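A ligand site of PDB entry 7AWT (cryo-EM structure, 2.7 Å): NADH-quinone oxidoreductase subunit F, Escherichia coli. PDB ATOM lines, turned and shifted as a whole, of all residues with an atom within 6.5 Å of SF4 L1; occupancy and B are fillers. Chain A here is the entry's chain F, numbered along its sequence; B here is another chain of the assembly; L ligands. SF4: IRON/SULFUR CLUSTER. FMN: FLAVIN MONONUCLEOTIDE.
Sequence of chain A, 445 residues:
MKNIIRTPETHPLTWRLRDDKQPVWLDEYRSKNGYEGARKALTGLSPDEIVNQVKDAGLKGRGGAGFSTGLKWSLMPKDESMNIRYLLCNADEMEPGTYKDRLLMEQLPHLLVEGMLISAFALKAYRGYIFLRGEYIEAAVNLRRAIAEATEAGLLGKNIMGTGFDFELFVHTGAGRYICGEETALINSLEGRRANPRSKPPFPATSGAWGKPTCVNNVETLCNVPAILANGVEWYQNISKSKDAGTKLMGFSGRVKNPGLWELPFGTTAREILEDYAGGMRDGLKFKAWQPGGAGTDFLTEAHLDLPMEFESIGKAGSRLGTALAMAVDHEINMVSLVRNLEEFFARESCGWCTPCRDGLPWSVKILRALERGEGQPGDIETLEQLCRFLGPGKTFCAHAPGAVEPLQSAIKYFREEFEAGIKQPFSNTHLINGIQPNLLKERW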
ATOM      1  N   ILE A 179      36.203  22.130 -17.446  1.00  0.00           N
ATOM      2  CA  ILE A 179      34.831  22.608 -17.425  1.00  0.00           C
ATOM      3  C   ILE A 179      34.559  23.611 -18.547  1.00  0.00           C
ATOM      4  O   ILE A 179      33.397  23.824 -18.905  1.00  0.00           O
ATOM      5  CB  ILE A 179      34.517  23.197 -16.038  1.00  0.00           C
ATOM      6  CG1 ILE A 179      33.019  23.462 -15.903  1.00  0.00           C
ATOM      7  CG2 ILE A 179      35.308  24.449 -15.796  1.00  0.00           C
ATOM      8  CD1 ILE A 179      32.169  22.227 -15.897  1.00  0.00           C
ATOM      9  N   ALA A 195      35.038  30.284 -15.929  1.00  0.00           N
ATOM     10  CA  ALA A 195      34.279  29.341 -16.741  1.00  0.00           C
ATOM     11  C   ALA A 195      33.206  28.670 -15.900  1.00  0.00           C
ATOM     12  O   ALA A 195      33.268  27.482 -15.574  1.00  0.00           O
ATOM     13  CB  ALA A 195      35.211  28.319 -17.374  1.00  0.00           C
ATOM     14  N   ASN A 196      32.193  29.450 -15.538  1.00  0.00           N
ATOM     15  CA  ASN A 196      31.075  28.818 -14.862  1.00  0.00           C
ATOM     16  C   ASN A 196      29.910  28.620 -15.812  1.00  0.00           C
ATOM     17  O   ASN A 196      29.577  29.532 -16.573  1.00  0.00           O
ATOM     18  CB  ASN A 196      30.609  29.660 -13.676  1.00  0.00           C
ATOM     19  CG  ASN A 196      31.420  29.418 -12.421  1.00  0.00           C
ATOM     20  OD1 ASN A 196      31.621  28.275 -12.010  1.00  0.00           O
ATOM     21  ND2 ASN A 196      31.900  30.490 -11.809  1.00  0.00           N
ATOM     22  N   PRO A 197      29.291  27.445 -15.823  1.00  0.00           N
ATOM     23  CA  PRO A 197      28.127  27.229 -16.684  1.00  0.00           C
ATOM     24  C   PRO A 197      27.024  28.231 -16.393  1.00  0.00           C
ATOM     25  O   PRO A 197      27.002  28.891 -15.348  1.00  0.00           O
ATOM     26  CB  PRO A 197      27.683  25.802 -16.329  1.00  0.00           C
ATOM     27  CG  PRO A 197      28.910  25.148 -15.859  1.00  0.00           C
ATOM     28  CD  PRO A 197      29.710  26.198 -15.153  1.00  0.00           C
ATOM     29  N   PHE A 346      37.363  14.186 -11.609  1.00  0.00           N
ATOM     30  CA  PHE A 346      36.062  14.839 -11.728  1.00  0.00           C
ATOM     31  C   PHE A 346      35.806  15.801 -10.581  1.00  0.00           C
ATOM     32  O   PHE A 346      34.999  16.724 -10.746  1.00  0.00           O
ATOM     33  CB  PHE A 346      34.950  13.794 -11.784  1.00  0.00           C
ATOM     34  CG  PHE A 346      34.707  13.249 -13.155  1.00  0.00           C
ATOM     35  CD1 PHE A 346      34.264  14.071 -14.162  1.00  0.00           C
ATOM     36  CD2 PHE A 346      34.910  11.915 -13.430  1.00  0.00           C
ATOM     37  CE1 PHE A 346      34.040  13.578 -15.426  1.00  0.00           C
ATOM     38  CE2 PHE A 346      34.691  11.421 -14.681  1.00  0.00           C
ATOM     39  CZ  PHE A 346      34.253  12.243 -15.675  1.00  0.00           C
ATOM     40  N   GLU A 349      38.563  18.920 -11.043  1.00  0.00           N
ATOM     41  CA  GLU A 349      38.317  19.579 -12.295  1.00  0.00           C
ATOM     42  C   GLU A 349      37.055  20.240 -12.451  1.00  0.00           C
ATOM     43  O   GLU A 349      36.699  20.688 -13.481  1.00  0.00           O
ATOM     44  CB  GLU A 349      38.387  18.675 -13.441  1.00  0.00           C
ATOM     45  CG  GLU A 349      38.927  19.504 -14.545  1.00  0.00           C
ATOM     46  CD  GLU A 349      40.372  19.737 -14.338  1.00  0.00           C
ATOM     47  OE1 GLU A 349      40.839  20.860 -14.241  1.00  0.00           O
ATOM     48  OE2 GLU A 349      41.086  18.777 -14.237  1.00  0.00           O
ATOM     49  N   SER A 350      36.369  20.318 -11.371  1.00  0.00           N
ATOM     50  CA  SER A 350      35.062  20.935 -11.337  1.00  0.00           C
ATOM     51  C   SER A 350      35.211  22.452 -11.214  1.00  0.00           C
ATOM     52  O   SER A 350      36.296  23.014 -11.373  1.00  0.00           O
ATOM     53  CB  SER A 350      34.239  20.369 -10.197  1.00  0.00           C
ATOM     54  OG  SER A 350      34.818  20.687  -8.949  1.00  0.00           O
ATOM     55  N   CYS A 351      34.106  23.115 -10.923  1.00  0.00           N
ATOM     56  CA  CYS A 351      34.122  24.531 -10.615  1.00  0.00           C
ATOM     57  C   CYS A 351      33.456  24.753  -9.256  1.00  0.00           C
ATOM     58  O   CYS A 351      33.096  23.810  -8.550  1.00  0.00           O
ATOM     59  CB  CYS A 351      33.452  25.340 -11.727  1.00  0.00           C
ATOM     60  SG  CYS A 351      31.651  25.255 -11.774  1.00  0.00           S
ATOM     61  N   GLY A 352      33.306  25.959  -8.797  1.00  0.00           N
ATOM     62  CA  GLY A 352      32.720  26.007  -7.483  1.00  0.00           C
ATOM     63  C   GLY A 352      31.264  26.340  -7.385  1.00  0.00           C
ATOM     64  O   GLY A 352      30.747  26.472  -6.307  1.00  0.00           O
ATOM     65  N   TRP A 353      30.581  26.440  -8.498  1.00  0.00           N
ATOM     66  CA  TRP A 353      29.224  26.899  -8.415  1.00  0.00           C
ATOM     67  C   TRP A 353      28.152  26.126  -7.658  1.00  0.00           C
ATOM     68  O   TRP A 353      27.508  26.689  -6.798  1.00  0.00           O
ATOM     69  CB  TRP A 353      28.742  27.194  -9.828  1.00  0.00           C
ATOM     70  CG  TRP A 353      27.547  27.994  -9.904  1.00  0.00           C
ATOM     71  CD1 TRP A 353      26.309  27.552 -10.096  1.00  0.00           C
ATOM     72  CD2 TRP A 353      27.459  29.411  -9.799  1.00  0.00           C
ATOM     73  NE1 TRP A 353      25.443  28.589 -10.127  1.00  0.00           N
ATOM     74  CE2 TRP A 353      26.134  29.745  -9.939  1.00  0.00           C
ATOM     75  CE3 TRP A 353      28.381  30.417  -9.598  1.00  0.00           C
ATOM     76  CZ2 TRP A 353      25.698  31.036  -9.879  1.00  0.00           C
ATOM     77  CZ3 TRP A 353      27.945  31.698  -9.538  1.00  0.00           C
ATOM     78  CH2 TRP A 353      26.619  32.001  -9.677  1.00  0.00           C
ATOM     79  N   CYS A 354      28.037  24.817  -7.839  1.00  0.00           N
ATOM     80  CA  CYS A 354      26.942  24.103  -7.217  1.00  0.00           C
ATOM     81  C   CYS A 354      27.380  23.142  -6.163  1.00  0.00           C
ATOM     82  O   CYS A 354      28.334  22.438  -6.346  1.00  0.00           O
ATOM     83  CB  CYS A 354      26.110  23.399  -8.280  1.00  0.00           C
ATOM     84  SG  CYS A 354      26.722  21.774  -8.697  1.00  0.00           S
ATOM     85  N   THR A 355      26.658  23.092  -5.061  1.00  0.00           N
ATOM     86  CA  THR A 355      27.067  22.244  -3.959  1.00  0.00           C
ATOM     87  C   THR A 355      27.130  20.755  -4.227  1.00  0.00           C
ATOM     88  O   THR A 355      28.042  20.103  -3.792  1.00  0.00           O
ATOM     89  CB  THR A 355      26.114  22.395  -2.796  1.00  0.00           C
ATOM     90  OG1 THR A 355      26.262  23.680  -2.235  1.00  0.00           O
ATOM     91  CG2 THR A 355      26.448  21.418  -1.756  1.00  0.00           C
ATOM     92  N   PRO A 356      26.167  20.202  -4.927  1.00  0.00           N
ATOM     93  CA  PRO A 356      26.272  18.754  -5.045  1.00  0.00           C
ATOM     94  C   PRO A 356      27.564  18.308  -5.677  1.00  0.00           C
ATOM     95  O   PRO A 356      28.189  17.451  -5.136  1.00  0.00           O
ATOM     96  CB  PRO A 356      25.124  18.406  -5.949  1.00  0.00           C
ATOM     97  CG  PRO A 356      24.143  19.473  -5.704  1.00  0.00           C
ATOM     98  CD  PRO A 356      24.944  20.704  -5.533  1.00  0.00           C
ATOM     99  N   CYS A 357      27.979  18.922  -6.765  1.00  0.00           N
ATOM    100  CA  CYS A 357      29.263  18.577  -7.371  1.00  0.00           C
ATOM    101  C   CYS A 357      30.412  18.965  -6.468  1.00  0.00           C
ATOM    102  O   CYS A 357      31.134  18.103  -5.948  1.00  0.00           O
ATOM    103  CB  CYS A 357      29.389  19.248  -8.737  1.00  0.00           C
ATOM    104  SG  CYS A 357      31.000  19.126  -9.509  1.00  0.00           S
ATOM    105  N   ARG A 358      30.560  20.265  -6.217  1.00  0.00           N
ATOM    106  CA  ARG A 358      31.749  20.797  -5.555  1.00  0.00           C
ATOM    107  C   ARG A 358      32.008  20.139  -4.209  1.00  0.00           C
ATOM    108  O   ARG A 358      33.154  19.877  -3.846  1.00  0.00           O
ATOM    109  CB  ARG A 358      31.618  22.307  -5.374  1.00  0.00           C
ATOM    110  CG  ARG A 358      32.242  22.824  -4.091  1.00  0.00           C
ATOM    111  CD  ARG A 358      32.313  24.334  -4.037  1.00  0.00           C
ATOM    112  NE  ARG A 358      30.990  24.940  -4.065  1.00  0.00           N
ATOM    113  CZ  ARG A 358      30.147  24.933  -3.032  1.00  0.00           C
ATOM    114  NH1 ARG A 358      30.483  24.349  -1.896  1.00  0.00           N
ATOM    115  NH2 ARG A 358      28.955  25.512  -3.153  1.00  0.00           N
ATOM    116  N   LEU A 361      31.605  15.484  -4.586  1.00  0.00           N
ATOM    117  CA  LEU A 361      32.603  14.699  -5.297  1.00  0.00           C
ATOM    118  C   LEU A 361      33.865  14.511  -4.442  1.00  0.00           C
ATOM    119  O   LEU A 361      34.418  13.407  -4.432  1.00  0.00           O
ATOM    120  CB  LEU A 361      32.926  15.342  -6.637  1.00  0.00           C
ATOM    121  CG  LEU A 361      31.925  15.015  -7.738  1.00  0.00           C
ATOM    122  CD1 LEU A 361      32.226  15.800  -8.995  1.00  0.00           C
ATOM    123  CD2 LEU A 361      31.925  13.538  -8.036  1.00  0.00           C
ATOM    124  N   THR A 396      22.121  18.930 -10.090  1.00  0.00           N
ATOM    125  CA  THR A 396      23.263  19.831 -10.180  1.00  0.00           C
ATOM    126  C   THR A 396      23.047  20.882 -11.256  1.00  0.00           C
ATOM    127  O   THR A 396      22.195  20.732 -12.140  1.00  0.00           O
ATOM    128  CB  THR A 396      24.542  19.051 -10.474  1.00  0.00           C
ATOM    129  OG1 THR A 396      24.372  18.336 -11.706  1.00  0.00           O
ATOM    130  CG2 THR A 396      24.815  18.058  -9.375  1.00  0.00           C
ATOM    131  N   PHE A 397      23.807  21.952 -11.198  1.00  0.00           N
ATOM    132  CA  PHE A 397      23.682  23.042 -12.134  1.00  0.00           C
ATOM    133  C   PHE A 397      24.033  22.721 -13.580  1.00  0.00           C
ATOM    134  O   PHE A 397      23.479  23.279 -14.485  1.00  0.00           O
ATOM    135  CB  PHE A 397      24.504  24.227 -11.655  1.00  0.00           C
ATOM    136  CG  PHE A 397      24.166  25.501 -12.332  1.00  0.00           C
ATOM    137  CD1 PHE A 397      23.065  26.204 -11.975  1.00  0.00           C
ATOM    138  CD2 PHE A 397      24.974  26.000 -13.300  1.00  0.00           C
ATOM    139  CE1 PHE A 397      22.748  27.378 -12.584  1.00  0.00           C
ATOM    140  CE2 PHE A 397      24.665  27.173 -13.928  1.00  0.00           C
ATOM    141  CZ  PHE A 397      23.559  27.867 -13.561  1.00  0.00           C
ATOM    142  N   CYS A 398      25.025  21.875 -13.784  1.00  0.00           N
ATOM    143  CA  CYS A 398      25.431  21.514 -15.138  1.00  0.00           C
ATOM    144  C   CYS A 398      25.530  20.026 -15.246  1.00  0.00           C
ATOM    145  O   CYS A 398      25.140  19.307 -14.363  1.00  0.00           O
ATOM    146  CB  CYS A 398      26.746  22.162 -15.524  1.00  0.00           C
ATOM    147  SG  CYS A 398      28.145  21.160 -15.049  1.00  0.00           S
ATOM    148  N   ALA A 399      26.040  19.544 -16.359  1.00  0.00           N
ATOM    149  CA  ALA A 399      26.125  18.125 -16.575  1.00  0.00           C
ATOM    150  C   ALA A 399      27.432  17.497 -16.157  1.00  0.00           C
ATOM    151  O   ALA A 399      27.679  16.370 -16.486  1.00  0.00           O
ATOM    152  CB  ALA A 399      25.858  17.811 -18.021  1.00  0.00           C
ATOM    153  N   HIS A 400      28.294  18.224 -15.466  1.00  0.00           N
ATOM    154  CA  HIS A 400      29.590  17.685 -15.090  1.00  0.00           C
ATOM    155  C   HIS A 400      29.468  16.608 -14.026  1.00  0.00           C
ATOM    156  O   HIS A 400      30.115  15.558 -14.118  1.00  0.00           O
ATOM    157  CB  HIS A 400      30.504  18.817 -14.599  1.00  0.00           C
ATOM    158  CG  HIS A 400      31.744  18.336 -13.909  1.00  0.00           C
ATOM    159  ND1 HIS A 400      32.826  17.828 -14.591  1.00  0.00           N
ATOM    160  CD2 HIS A 400      32.087  18.315 -12.603  1.00  0.00           C
ATOM    161  CE1 HIS A 400      33.774  17.493 -13.733  1.00  0.00           C
ATOM    162  NE2 HIS A 400      33.343  17.783 -12.521  1.00  0.00           N
ATOM    163  N   ALA A 401      28.640  16.851 -13.007  1.00  0.00           N
ATOM    164  CA  ALA A 401      28.468  15.846 -11.947  1.00  0.00           C
ATOM    165  C   ALA A 401      27.590  14.685 -12.375  1.00  0.00           C
ATOM    166  O   ALA A 401      27.902  13.537 -12.012  1.00  0.00           O
ATOM    167  CB  ALA A 401      27.939  16.522 -10.684  1.00  0.00           C
ATOM    168  N   PRO A 402      26.471  14.879 -13.087  1.00  0.00           N
ATOM    169  CA  PRO A 402      25.709  13.722 -13.573  1.00  0.00           C
ATOM    170  C   PRO A 402      26.539  12.732 -14.342  1.00  0.00           C
ATOM    171  O   PRO A 402      26.298  11.522 -14.243  1.00  0.00           O
ATOM    172  CB  PRO A 402      24.648  14.371 -14.473  1.00  0.00           C
ATOM    173  CG  PRO A 402      24.423  15.683 -13.865  1.00  0.00           C
ATOM    174  CD  PRO A 402      25.751  16.136 -13.367  1.00  0.00           C
ATOM    175  N   ALA B  44      22.863  28.309  -7.792  1.00  0.00           N
ATOM    176  CA  ALA B  44      24.085  27.797  -7.253  1.00  0.00           C
ATOM    177  C   ALA B  44      24.147  26.884  -6.099  1.00  0.00           C
ATOM    178  O   ALA B  44      24.685  25.847  -6.241  1.00  0.00           O
ATOM    179  CB  ALA B  44      24.935  28.979  -6.860  1.00  0.00           C
HETATM  180 FE1  SF4 L   1      30.276  23.476 -11.505  1.00  0.00          FE
HETATM  181 FE2  SF4 L   1      30.258  20.816 -10.830  1.00  0.00          FE
HETATM  182 FE3  SF4 L   1      28.817  21.699 -12.984  1.00  0.00          FE
HETATM  183 FE4  SF4 L   1      28.028  22.338 -10.452  1.00  0.00          FE
HETATM  184  S1  SF4 L   1      28.123  20.266 -11.356  1.00  0.00           S
HETATM  185  S2  SF4 L   1      28.161  23.743 -12.228  1.00  0.00           S
HETATM  186  S3  SF4 L   1      30.044  22.572  -9.430  1.00  0.00           S
HETATM  187  S4  SF4 L   1      31.069  21.739 -12.749  1.00  0.00           S
HETATM  188  N1  FMN L   2      32.082  18.877 -26.041  1.00  0.00           N
HETATM  189  C2  FMN L   2      33.251  18.865 -26.757  1.00  0.00           C
HETATM  190  O2  FMN L   2      33.207  18.876 -27.969  1.00  0.00           O
HETATM  191  N3  FMN L   2      34.466  18.855 -26.118  1.00  0.00           N
HETATM  192  C4  FMN L   2      34.502  18.858 -24.746  1.00  0.00           C
HETATM  193  O4  FMN L   2      35.558  18.844 -24.147  1.00  0.00           O
HETATM  194  C4A FMN L   2      33.319  18.861 -24.025  1.00  0.00           C
HETATM  195  N5  FMN L   2      33.382  18.852 -22.662  1.00  0.00           N
HETATM  196  C5A FMN L   2      32.226  18.864 -21.929  1.00  0.00           C
HETATM  197  C6  FMN L   2      32.352  18.863 -20.559  1.00  0.00           C
HETATM  198  C7  FMN L   2      31.211  18.865 -19.786  1.00  0.00           C
HETATM  199  C7M FMN L   2      31.354  18.865 -18.309  1.00  0.00           C
HETATM  200  C8  FMN L   2      29.958  18.887 -20.388  1.00  0.00           C
HETATM  201  C8M FMN L   2      28.715  18.884 -19.562  1.00  0.00           C
HETATM  202  C9  FMN L   2      29.850  18.887 -21.772  1.00  0.00           C
HETATM  203  C9A FMN L   2      30.995  18.875 -22.554  1.00  0.00           C
HETATM  204  N10 FMN L   2      30.932  18.893 -23.939  1.00  0.00           N
HETATM  205  C10 FMN L   2      32.096  18.871 -24.668  1.00  0.00           C
HETATM  206  C1' FMN L   2      29.617  18.915 -24.669  1.00  0.00           C
HETATM  207  C2' FMN L   2      29.277  20.386 -24.947  1.00  0.00           C
HETATM  208  O2' FMN L   2      28.516  20.908 -23.885  1.00  0.00           O
HETATM  209  C3' FMN L   2      28.510  20.636 -26.248  1.00  0.00           C
HETATM  210  O3' FMN L   2      27.323  19.885 -26.239  1.00  0.00           O
HETATM  211  C4' FMN L   2      29.363  20.258 -27.449  1.00  0.00           C
HETATM  212  O4' FMN L   2      30.685  20.696 -27.273  1.00  0.00           O
HETATM  213  C5' FMN L   2      28.835  20.868 -28.741  1.00  0.00           C
HETATM  214  O5' FMN L   2      27.564  20.327 -28.988  1.00  0.00           O
HETATM  215  P   FMN L   2      27.380  19.252 -30.169  1.00  0.00           P
HETATM  216  O1P FMN L   2      27.787  17.914 -29.622  1.00  0.00           O
HETATM  217  O2P FMN L   2      25.946  19.225 -30.621  1.00  0.00           O
HETATM  218  O3P FMN L   2      28.275  19.605 -31.311  1.00  0.00           O
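FE3 of SF4 L1 is bound by SG of Cys 398 (2.2 Å). N of Cys 354 sits close to S3 of SF4 L1 (3.4 Å). FE4 of SF4 L1 is bound by SG of Cys 354, 2.3 Å away. The side-chain sulfur of Cys 351 is bound to an iron atom (FE1) of SF4 L1 (2.3 Å). An iron atom (FE2) of SF4 L1 is bound by the side-chain sulfur of Cys 357 (2.3 Å).
N of His 400 lies close to SG of Cys 398 (3.0 Å). The side-chain hydroxyl of Thr 396 is in hydrogen-bond range of the backbone carbonyl oxygen of Cys 398, 2.9 Å away. SG of Cys 354 lies close to N of Cys 357 (3.7 Å). The backbone NH of Trp 353 lies close to the side-chain sulfur of Cys 351 (3.6 Å). The side-chain amide oxygen (OD1) of Asn 196 lies close to the side-chain sulfur (SG) of Cys 351 (3.0 Å). A ring nitrogen (NE2) of His 400 sits at hydrogen-bond distance from the backbone carbonyl oxygen (O) of Phe 346. The guanidinium group of Arg 358 sits at hydrogen-bond distance from the backbone carbonyl oxygen of Gly 352 (2.7 Å). The side-chain hydroxyl of Thr 355 sits at hydrogen-bond distance from the guanidinium group of Arg 358 (3.4 Å).
CD1 of Ile 179 touches S4 of SF4 L1, 3.4 Å away. Pro 197 touches SF4 L1. N of Arg 358 touches S3 of SF4 L1 (3.99 Å). CB of Thr 396 touches S1 of SF4 L1 (3.9 Å). Phe 397 touches SF4 L1. His 400 touches SF4 L1. CB of Ala 401 touches S1 of SF4 L1, 3.8 Å away. Of the 24 residues printed, 11 come within 4 Å of SF4 L1. The nearest printed residue that does not touch SF4 L1 is Trp 353 (4.01 Å).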
